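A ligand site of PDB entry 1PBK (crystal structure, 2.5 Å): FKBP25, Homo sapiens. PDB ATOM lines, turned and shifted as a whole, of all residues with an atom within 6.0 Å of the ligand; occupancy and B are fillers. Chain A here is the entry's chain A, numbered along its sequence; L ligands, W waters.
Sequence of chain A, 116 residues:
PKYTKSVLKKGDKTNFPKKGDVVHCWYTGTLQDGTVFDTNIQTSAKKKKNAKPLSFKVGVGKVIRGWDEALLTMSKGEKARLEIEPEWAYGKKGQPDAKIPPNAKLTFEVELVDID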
ATOM      1  N   TYR A  27      14.514 -14.456  17.637  1.00  0.00           N
ATOM      2  CA  TYR A  27      13.542 -13.689  16.888  1.00  0.00           C
ATOM      3  C   TYR A  27      14.043 -12.300  16.546  1.00  0.00           C
ATOM      4  O   TYR A  27      14.971 -11.768  17.166  1.00  0.00           O
ATOM      5  CB  TYR A  27      12.246 -13.532  17.664  1.00  0.00           C
ATOM      6  CG  TYR A  27      12.283 -12.663  18.911  1.00  0.00           C
ATOM      7  CD1 TYR A  27      12.632 -13.242  20.144  1.00  0.00           C
ATOM      8  CD2 TYR A  27      11.978 -11.313  18.834  1.00  0.00           C
ATOM      9  CE1 TYR A  27      12.699 -12.447  21.301  1.00  0.00           C
ATOM     10  CE2 TYR A  27      12.047 -10.516  19.981  1.00  0.00           C
ATOM     11  CZ  TYR A  27      12.423 -11.102  21.189  1.00  0.00           C
ATOM     12  OH  TYR A  27      12.511 -10.305  22.289  1.00  0.00           O
ATOM     13  N   GLY A  29      11.736  -8.628  15.385  1.00  0.00           N
ATOM     14  CA  GLY A  29      10.443  -8.123  15.078  1.00  0.00           C
ATOM     15  C   GLY A  29      10.609  -6.793  14.390  1.00  0.00           C
ATOM     16  O   GLY A  29      11.425  -5.962  14.834  1.00  0.00           O
ATOM     17  N   PHE A  37      11.896  -3.335  15.747  1.00  0.00           N
ATOM     18  CA  PHE A  37      11.642  -2.785  17.064  1.00  0.00           C
ATOM     19  C   PHE A  37      12.304  -3.651  18.131  1.00  0.00           C
ATOM     20  O   PHE A  37      12.419  -3.190  19.271  1.00  0.00           O
ATOM     21  CB  PHE A  37      10.137  -2.619  17.384  1.00  0.00           C
ATOM     22  CG  PHE A  37       9.317  -3.903  17.340  1.00  0.00           C
ATOM     23  CD1 PHE A  37       9.326  -4.793  18.411  1.00  0.00           C
ATOM     24  CD2 PHE A  37       8.621  -4.227  16.180  1.00  0.00           C
ATOM     25  CE1 PHE A  37       8.691  -6.034  18.299  1.00  0.00           C
ATOM     26  CE2 PHE A  37       7.968  -5.456  16.098  1.00  0.00           C
ATOM     27  CZ  PHE A  37       8.014  -6.370  17.143  1.00  0.00           C
ATOM     28  N   ASP A  38      12.713  -4.897  17.845  1.00  0.00           N
ATOM     29  CA  ASP A  38      13.310  -5.744  18.855  1.00  0.00           C
ATOM     30  C   ASP A  38      13.962  -6.952  18.201  1.00  0.00           C
ATOM     31  O   ASP A  38      13.459  -7.395  17.177  1.00  0.00           O
ATOM     32  CB  ASP A  38      12.260  -6.178  19.885  1.00  0.00           C
ATOM     33  CG  ASP A  38      12.790  -6.883  21.135  1.00  0.00           C
ATOM     34  OD1 ASP A  38      14.001  -6.991  21.324  1.00  0.00           O
ATOM     35  OD2 ASP A  38      11.995  -7.334  21.948  1.00  0.00           O
ATOM     36  N   LEU A  54      14.934 -17.004  23.733  1.00  0.00           N
ATOM     37  CA  LEU A  54      13.722 -16.807  24.519  1.00  0.00           C
ATOM     38  C   LEU A  54      13.168 -18.170  24.893  1.00  0.00           C
ATOM     39  O   LEU A  54      13.323 -19.141  24.134  1.00  0.00           O
ATOM     40  CB  LEU A  54      12.757 -16.046  23.665  1.00  0.00           C
ATOM     41  CG  LEU A  54      11.524 -15.580  24.369  1.00  0.00           C
ATOM     42  CD1 LEU A  54      11.799 -14.384  25.257  1.00  0.00           C
ATOM     43  CD2 LEU A  54      10.566 -15.186  23.280  1.00  0.00           C
ATOM     44  N   SER A  55      12.581 -18.290  26.078  1.00  0.00           N
ATOM     45  CA  SER A  55      12.003 -19.552  26.517  1.00  0.00           C
ATOM     46  C   SER A  55      10.677 -19.188  27.144  1.00  0.00           C
ATOM     47  O   SER A  55      10.543 -18.131  27.777  1.00  0.00           O
ATOM     48  CB  SER A  55      12.879 -20.217  27.543  1.00  0.00           C
ATOM     49  OG  SER A  55      14.134 -20.496  26.933  1.00  0.00           O
ATOM     50  N   PHE A  56       9.693 -20.017  26.844  1.00  0.00           N
ATOM     51  CA  PHE A  56       8.352 -19.871  27.374  1.00  0.00           C
ATOM     52  C   PHE A  56       7.664 -21.201  27.126  1.00  0.00           C
ATOM     53  O   PHE A  56       8.254 -22.120  26.529  1.00  0.00           O
ATOM     54  CB  PHE A  56       7.573 -18.673  26.758  1.00  0.00           C
ATOM     55  CG  PHE A  56       7.501 -18.646  25.225  1.00  0.00           C
ATOM     56  CD1 PHE A  56       8.583 -18.161  24.476  1.00  0.00           C
ATOM     57  CD2 PHE A  56       6.365 -19.152  24.563  1.00  0.00           C
ATOM     58  CE1 PHE A  56       8.558 -18.247  23.094  1.00  0.00           C
ATOM     59  CE2 PHE A  56       6.351 -19.232  23.174  1.00  0.00           C
ATOM     60  CZ  PHE A  56       7.446 -18.798  22.440  1.00  0.00           C
ATOM     61  N   GLY A  61      -0.578 -19.143  26.475  1.00  0.00           N
ATOM     62  CA  GLY A  61      -0.916 -17.722  26.592  1.00  0.00           C
ATOM     63  C   GLY A  61       0.185 -16.897  27.261  1.00  0.00           C
ATOM     64  O   GLY A  61      -0.015 -15.761  27.659  1.00  0.00           O
ATOM     65  N   LYS A  62       1.380 -17.459  27.373  1.00  0.00           N
ATOM     66  CA  LYS A  62       2.518 -16.690  27.810  1.00  0.00           C
ATOM     67  C   LYS A  62       2.918 -15.644  26.776  1.00  0.00           C
ATOM     68  O   LYS A  62       3.429 -14.588  27.145  1.00  0.00           O
ATOM     69  CB  LYS A  62       3.684 -17.599  28.092  1.00  0.00           C
ATOM     70  CG  LYS A  62       3.475 -18.623  29.204  1.00  0.00           C
ATOM     71  CD  LYS A  62       3.471 -18.075  30.643  1.00  0.00           C
ATOM     72  CE  LYS A  62       2.197 -17.360  31.097  1.00  0.00           C
ATOM     73  NZ  LYS A  62       2.350 -16.749  32.412  1.00  0.00           N
ATOM     74  N   VAL A  63       2.686 -15.859  25.491  1.00  0.00           N
ATOM     75  CA  VAL A  63       3.067 -14.930  24.430  1.00  0.00           C
ATOM     76  C   VAL A  63       1.817 -14.508  23.666  1.00  0.00           C
ATOM     77  O   VAL A  63       0.730 -15.058  23.895  1.00  0.00           O
ATOM     78  CB  VAL A  63       4.114 -15.529  23.461  1.00  0.00           C
ATOM     79  CG1 VAL A  63       5.425 -15.631  24.174  1.00  0.00           C
ATOM     80  CG2 VAL A  63       3.738 -16.910  22.963  1.00  0.00           C
ATOM     81  N   ILE A  64       1.949 -13.535  22.766  1.00  0.00           N
ATOM     82  CA  ILE A  64       0.844 -13.094  21.919  1.00  0.00           C
ATOM     83  C   ILE A  64       0.271 -14.238  21.084  1.00  0.00           C
ATOM     84  O   ILE A  64       0.996 -15.160  20.682  1.00  0.00           O
ATOM     85  CB  ILE A  64       1.256 -11.925  20.974  1.00  0.00           C
ATOM     86  CG1 ILE A  64       2.465 -12.169  20.084  1.00  0.00           C
ATOM     87  CG2 ILE A  64       1.371 -10.662  21.789  1.00  0.00           C
ATOM     88  CD1 ILE A  64       2.723 -10.978  19.153  1.00  0.00           C
ATOM     89  N   TRP A  67       1.968 -15.836  17.969  1.00  0.00           N
ATOM     90  CA  TRP A  67       3.125 -16.670  18.284  1.00  0.00           C
ATOM     91  C   TRP A  67       2.715 -18.019  18.837  1.00  0.00           C
ATOM     92  O   TRP A  67       3.213 -19.091  18.460  1.00  0.00           O
ATOM     93  CB  TRP A  67       3.975 -15.968  19.314  1.00  0.00           C
ATOM     94  CG  TRP A  67       5.146 -15.221  18.723  1.00  0.00           C
ATOM     95  CD1 TRP A  67       4.970 -14.041  18.039  1.00  0.00           C
ATOM     96  CD2 TRP A  67       6.453 -15.586  18.870  1.00  0.00           C
ATOM     97  NE1 TRP A  67       6.193 -13.641  17.756  1.00  0.00           N
ATOM     98  CE2 TRP A  67       7.105 -14.510  18.249  1.00  0.00           C
ATOM     99  CE3 TRP A  67       7.186 -16.568  19.556  1.00  0.00           C
ATOM    100  CZ2 TRP A  67       8.492 -14.392  18.361  1.00  0.00           C
ATOM    101  CZ3 TRP A  67       8.589 -16.451  19.629  1.00  0.00           C
ATOM    102  CH2 TRP A  67       9.228 -15.361  19.049  1.00  0.00           C
ATOM    103  N   TYR A  90      -0.959  -6.860  19.696  1.00  0.00           N
ATOM    104  CA  TYR A  90      -1.260  -5.936  20.775  1.00  0.00           C
ATOM    105  C   TYR A  90      -2.500  -5.095  20.503  1.00  0.00           C
ATOM    106  O   TYR A  90      -2.873  -4.222  21.278  1.00  0.00           O
ATOM    107  CB  TYR A  90      -0.022  -5.093  21.159  1.00  0.00           C
ATOM    108  CG  TYR A  90       1.127  -5.981  21.608  1.00  0.00           C
ATOM    109  CD1 TYR A  90       1.155  -6.512  22.898  1.00  0.00           C
ATOM    110  CD2 TYR A  90       2.156  -6.276  20.721  1.00  0.00           C
ATOM    111  CE1 TYR A  90       2.230  -7.315  23.311  1.00  0.00           C
ATOM    112  CE2 TYR A  90       3.222  -7.096  21.118  1.00  0.00           C
ATOM    113  CZ  TYR A  90       3.259  -7.587  22.418  1.00  0.00           C
ATOM    114  OH  TYR A  90       4.324  -8.338  22.807  1.00  0.00           O
ATOM    115  N   GLN A  95       1.194  -1.246  22.536  1.00  0.00           N
ATOM    116  CA  GLN A  95       1.906  -1.277  23.793  1.00  0.00           C
ATOM    117  C   GLN A  95       2.930  -0.182  23.700  1.00  0.00           C
ATOM    118  O   GLN A  95       4.103  -0.446  23.439  1.00  0.00           O
ATOM    119  CB  GLN A  95       2.521  -2.650  24.025  1.00  0.00           C
ATOM    120  CG  GLN A  95       2.577  -3.003  25.504  1.00  0.00           C
ATOM    121  CD  GLN A  95       1.251  -2.899  26.251  1.00  0.00           C
ATOM    122  OE1 GLN A  95       0.267  -3.589  25.988  1.00  0.00           O
ATOM    123  NE2 GLN A  95       1.165  -2.042  27.261  1.00  0.00           N
ATOM    124  N   ALA A  98       6.432  -0.202  25.237  1.00  0.00           N
ATOM    125  CA  ALA A  98       7.291  -1.227  24.653  1.00  0.00           C
ATOM    126  C   ALA A  98       7.566  -1.058  23.148  1.00  0.00           C
ATOM    127  O   ALA A  98       7.981  -2.013  22.485  1.00  0.00           O
ATOM    128  CB  ALA A  98       6.582  -2.554  24.896  1.00  0.00           C
ATOM    129  N   LYS A  99       7.346   0.140  22.582  1.00  0.00           N
ATOM    130  CA  LYS A  99       7.574   0.501  21.183  1.00  0.00           C
ATOM    131  C   LYS A  99       6.534  -0.047  20.213  1.00  0.00           C
ATOM    132  O   LYS A  99       6.796  -0.173  19.008  1.00  0.00           O
ATOM    133  CB  LYS A  99       8.945   0.082  20.621  1.00  0.00           C
ATOM    134  CG  LYS A  99      10.149   0.416  21.471  1.00  0.00           C
ATOM    135  CD  LYS A  99      11.415  -0.149  20.832  1.00  0.00           C
ATOM    136  CE  LYS A  99      12.487  -0.192  21.912  1.00  0.00           C
ATOM    137  NZ  LYS A  99      13.769  -0.667  21.410  1.00  0.00           N
ATOM    138  N   ILE A 100       5.334  -0.423  20.654  1.00  0.00           N
ATOM    139  CA  ILE A 100       4.356  -1.018  19.755  1.00  0.00           C
ATOM    140  C   ILE A 100       3.250   0.011  19.513  1.00  0.00           C
ATOM    141  O   ILE A 100       2.478   0.286  20.436  1.00  0.00           O
ATOM    142  CB  ILE A 100       3.774  -2.330  20.310  1.00  0.00           C
ATOM    143  CG1 ILE A 100       4.817  -3.341  20.718  1.00  0.00           C
ATOM    144  CG2 ILE A 100       2.830  -2.949  19.301  1.00  0.00           C
ATOM    145  CD1 ILE A 100       5.773  -3.711  19.565  1.00  0.00           C
ATOM    146  N   LEU A 106       2.466  -6.802  12.740  1.00  0.00           N
ATOM    147  CA  LEU A 106       3.846  -6.939  13.171  1.00  0.00           C
ATOM    148  C   LEU A 106       4.474  -8.067  12.420  1.00  0.00           C
ATOM    149  O   LEU A 106       3.770  -9.044  12.202  1.00  0.00           O
ATOM    150  CB  LEU A 106       3.918  -7.283  14.656  1.00  0.00           C
ATOM    151  CG  LEU A 106       3.439  -6.231  15.615  1.00  0.00           C
ATOM    152  CD1 LEU A 106       3.400  -6.805  17.016  1.00  0.00           C
ATOM    153  CD2 LEU A 106       4.332  -5.029  15.537  1.00  0.00           C
ATOM    154  N   PHE A 108       7.568 -10.933  12.241  1.00  0.00           N
ATOM    155  CA  PHE A 108       8.578 -11.514  13.078  1.00  0.00           C
ATOM    156  C   PHE A 108       9.285 -12.545  12.260  1.00  0.00           C
ATOM    157  O   PHE A 108       8.639 -13.291  11.532  1.00  0.00           O
ATOM    158  CB  PHE A 108       7.986 -12.257  14.262  1.00  0.00           C
ATOM    159  CG  PHE A 108       7.589 -11.358  15.405  1.00  0.00           C
ATOM    160  CD1 PHE A 108       8.516 -11.019  16.389  1.00  0.00           C
ATOM    161  CD2 PHE A 108       6.288 -10.852  15.464  1.00  0.00           C
ATOM    162  CE1 PHE A 108       8.148 -10.136  17.420  1.00  0.00           C
ATOM    163  CE2 PHE A 108       5.919  -9.992  16.502  1.00  0.00           C
ATOM    164  CZ  PHE A 108       6.855  -9.625  17.483  1.00  0.00           C
HETATM  165  C1  LIG L   1       5.524 -11.537  23.264  1.00  0.00           C
HETATM  166  O1  LIG L   1       6.015 -10.976  24.484  1.00  0.00           O
HETATM  167  O2  LIG L   1       4.524 -12.242  23.288  1.00  0.00           O
HETATM  168  C2  LIG L   1       6.170 -11.309  21.914  1.00  0.00           C
HETATM  169  C3  LIG L   1       6.465 -12.642  21.264  1.00  0.00           C
HETATM  170  C4  LIG L   1       7.695 -13.341  21.813  1.00  0.00           C
HETATM  171  C5  LIG L   1       8.890 -12.378  21.838  1.00  0.00           C
HETATM  172  C6  LIG L   1       8.520 -11.129  22.621  1.00  0.00           C
HETATM  173  N1  LIG L   1       7.402 -10.511  21.909  1.00  0.00           N
HETATM  174  C7  LIG L   1       7.378  -9.196  21.576  1.00  0.00           C
HETATM  175  O3  LIG L   1       6.356  -8.687  21.103  1.00  0.00           O
HETATM  176  C8  LIG L   1       8.532  -8.398  21.581  1.00  0.00           C
HETATM  177  O4  LIG L   1       9.335  -8.585  20.662  1.00  0.00           O
HETATM  178  C9  LIG L   1       8.885  -7.440  22.731  1.00  0.00           C
HETATM  179  O5  LIG L   1       9.650  -8.287  23.567  1.00  0.00           O
HETATM  180  O6  LIG L   1       9.579  -6.283  22.285  1.00  0.00           O
HETATM  181  C10 LIG L   1       7.635  -6.878  23.427  1.00  0.00           C
HETATM  182  C11 LIG L   1       7.954  -6.413  24.825  1.00  0.00           C
HETATM  183  C12 LIG L   1       8.767  -7.441  25.629  1.00  0.00           C
HETATM  184  C13 LIG L   1      10.005  -7.928  24.881  1.00  0.00           C
HETATM  185  C14 LIG L   1      10.575  -9.160  25.548  1.00  0.00           C
HETATM  186  C15 LIG L   1      11.343  -8.865  26.849  1.00  0.00           C
HETATM  187  O7  LIG L   1      12.564  -8.383  26.445  1.00  0.00           O
HETATM  188  C16 LIG L   1      11.538 -10.096  27.719  1.00  0.00           C
HETATM  189  C17 LIG L   1      10.823 -10.198  28.830  1.00  0.00           C
HETATM  190  C18 LIG L   1      10.859 -11.339  29.746  1.00  0.00           C
HETATM  191  C19 LIG L   1      10.105 -11.348  30.842  1.00  0.00           C
HETATM  192  C20 LIG L   1      10.089 -12.566  31.666  1.00  0.00           C
HETATM  193  C21 LIG L   1       9.328 -12.685  32.730  1.00  0.00           C
HETATM  194  C22 LIG L   1       9.196 -13.950  33.576  1.00  0.00           C
HETATM  195  C23 LIG L   1       7.758 -14.416  33.470  1.00  0.00           C
HETATM  196  C24 LIG L   1       7.211 -14.704  32.095  1.00  0.00           C
HETATM  197  C25 LIG L   1       5.704 -14.875  32.214  1.00  0.00           C
HETATM  198  O8  LIG L   1       5.220 -15.939  32.610  1.00  0.00           O
HETATM  199  C26 LIG L   1       4.818 -13.677  31.874  1.00  0.00           C
HETATM  200  O9  LIG L   1       3.534 -14.033  32.274  1.00  0.00           O
HETATM  201  C27 LIG L   1       4.678 -13.351  30.367  1.00  0.00           C
HETATM  202  O10 LIG L   1       4.275 -14.560  29.736  1.00  0.00           O
HETATM  203  C28 LIG L   1       5.934 -12.774  29.695  1.00  0.00           C
HETATM  204  C29 LIG L   1       6.656 -13.478  28.805  1.00  0.00           C
HETATM  205  C30 LIG L   1       7.853 -12.981  28.028  1.00  0.00           C
HETATM  206  C31 LIG L   1       7.422 -12.426  26.662  1.00  0.00           C
HETATM  207  O11 LIG L   1       7.667 -12.997  25.590  1.00  0.00           O
HETATM  208  C32 LIG L   1       6.662 -11.108  26.632  1.00  0.00           C
HETATM  209  C33 LIG L   1       5.460 -11.147  25.732  1.00  0.00           C
HETATM  210  C34 LIG L   1       4.435 -10.007  25.902  1.00  0.00           C
HETATM  211  C35 LIG L   1       3.504 -10.218  27.070  1.00  0.00           C
HETATM  212  C36 LIG L   1       2.276 -11.107  26.986  1.00  0.00           C
HETATM  213  C37 LIG L   1       1.786 -11.475  28.373  1.00  0.00           C
HETATM  214  C38 LIG L   1       0.623 -12.466  28.341  1.00  0.00           C
HETATM  215  O12 LIG L   1       0.111 -12.634  29.602  1.00  0.00           O
HETATM  216  C39 LIG L   1      -0.560 -11.990  27.479  1.00  0.00           C
HETATM  217  O13 LIG L   1      -1.321 -13.178  27.290  1.00  0.00           O
HETATM  218  C40 LIG L   1      -0.124 -11.375  26.133  1.00  0.00           C
HETATM  219  C41 LIG L   1       1.113 -10.457  26.214  1.00  0.00           C
HETATM  220  C42 LIG L   1       6.974  -5.735  22.654  1.00  0.00           C
HETATM  221  C43 LIG L   1      12.571 -11.121  27.257  1.00  0.00           C
HETATM  222  C44 LIG L   1       9.404 -13.659  35.026  1.00  0.00           C
HETATM  223  C45 LIG L   1       7.828 -15.958  31.475  1.00  0.00           C
HETATM  224  C46 LIG L   1       6.283 -11.361  30.148  1.00  0.00           C
HETATM  225  C47 LIG L   1       8.814 -14.137  27.827  1.00  0.00           C
HETATM  226  C48 LIG L   1       5.116  -8.670  26.128  1.00  0.00           C
HETATM  227  C49 LIG L   1      13.200  -7.482  27.273  1.00  0.00           C
HETATM  228  C50 LIG L   1       3.146 -13.244  33.314  1.00  0.00           C
HETATM  229  C51 LIG L   1       0.485 -13.844  30.167  1.00  0.00           C
HETATM  230  O   HOH W   1      10.512  -3.484  22.757  1.00  0.00           O
HETATM  231  O   HOH W   2      14.553  -8.291  24.041  1.00  0.00           O
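The side-chain carboxylate (OD2) of Asp 38 is in hydrogen-bond range of the side-chain hydroxyl (OH) of Tyr 27 (3.0 Å). The backbone carbonyl oxygen (O) of Asp 38 lies within hydrogen-bond range of the backbone NH (N) of Gly 29. N of Phe 37 sits at hydrogen-bond distance from O of Gly 29 (2.8 Å). O of Ile 100 lies within hydrogen-bond range of N of Gln 95, 2.9 Å away.
O6 of the ligand sits at hydrogen-bond distance from OD2 of Asp 38, 2.7 Å away. The side-chain hydroxyl (OH) of Tyr 90 is in hydrogen-bond range of an oxygen (O3) of the ligand, at 2.7 Å. O of Lys 62 sits at hydrogen-bond distance from O10 of the ligand (2.7 Å). An oxygen (O9) of the ligand lies within hydrogen-bond range of the side-chain amino group (NZ) of Lys 62. The backbone carbonyl oxygen (O) of Gly 61 sits at hydrogen-bond distance from an oxygen (O13) of the ligand (2.9 Å). O2 of the ligand sits at hydrogen-bond distance from N of Ile 64 (2.9 Å).
Water W1 bridges the backbone carbonyl oxygen of Ala 98 and an oxygen (O6) of the ligand. Water W2 lies within hydrogen-bond range of OD1 of Asp 38 (3.1 Å), O7 of the ligand (3.1 Å) and OH of Tyr 27 (3.4 Å).
Tyr 27 touches the ligand. CE1 of Phe 37 touches O4 of the ligand, 3.5 Å away. CD2 of Leu 54 touches C5 of the ligand (3.6 Å). Val 63 touches the ligand. CE2 of Trp 67 touches C3 of the ligand, 3.6 Å away. O of Ala 98 touches C42 of the ligand, 3.9 Å away. Ile 100 touches the ligand (CG1 to C42, 3.8 Å). Phe 108 touches the ligand (CZ to O3, 3.8 Å). Hydrophobic or aromatic side chains within 4 Å of the ligand: Tyr 27, Phe 37, Leu 54, Val 63, Ile 64, Trp 67, Tyr 90, Ala 98, Ile 100 and Phe 108. The nearest printed residue that does not touch the ligand is Ser 55 (4.4 Å).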
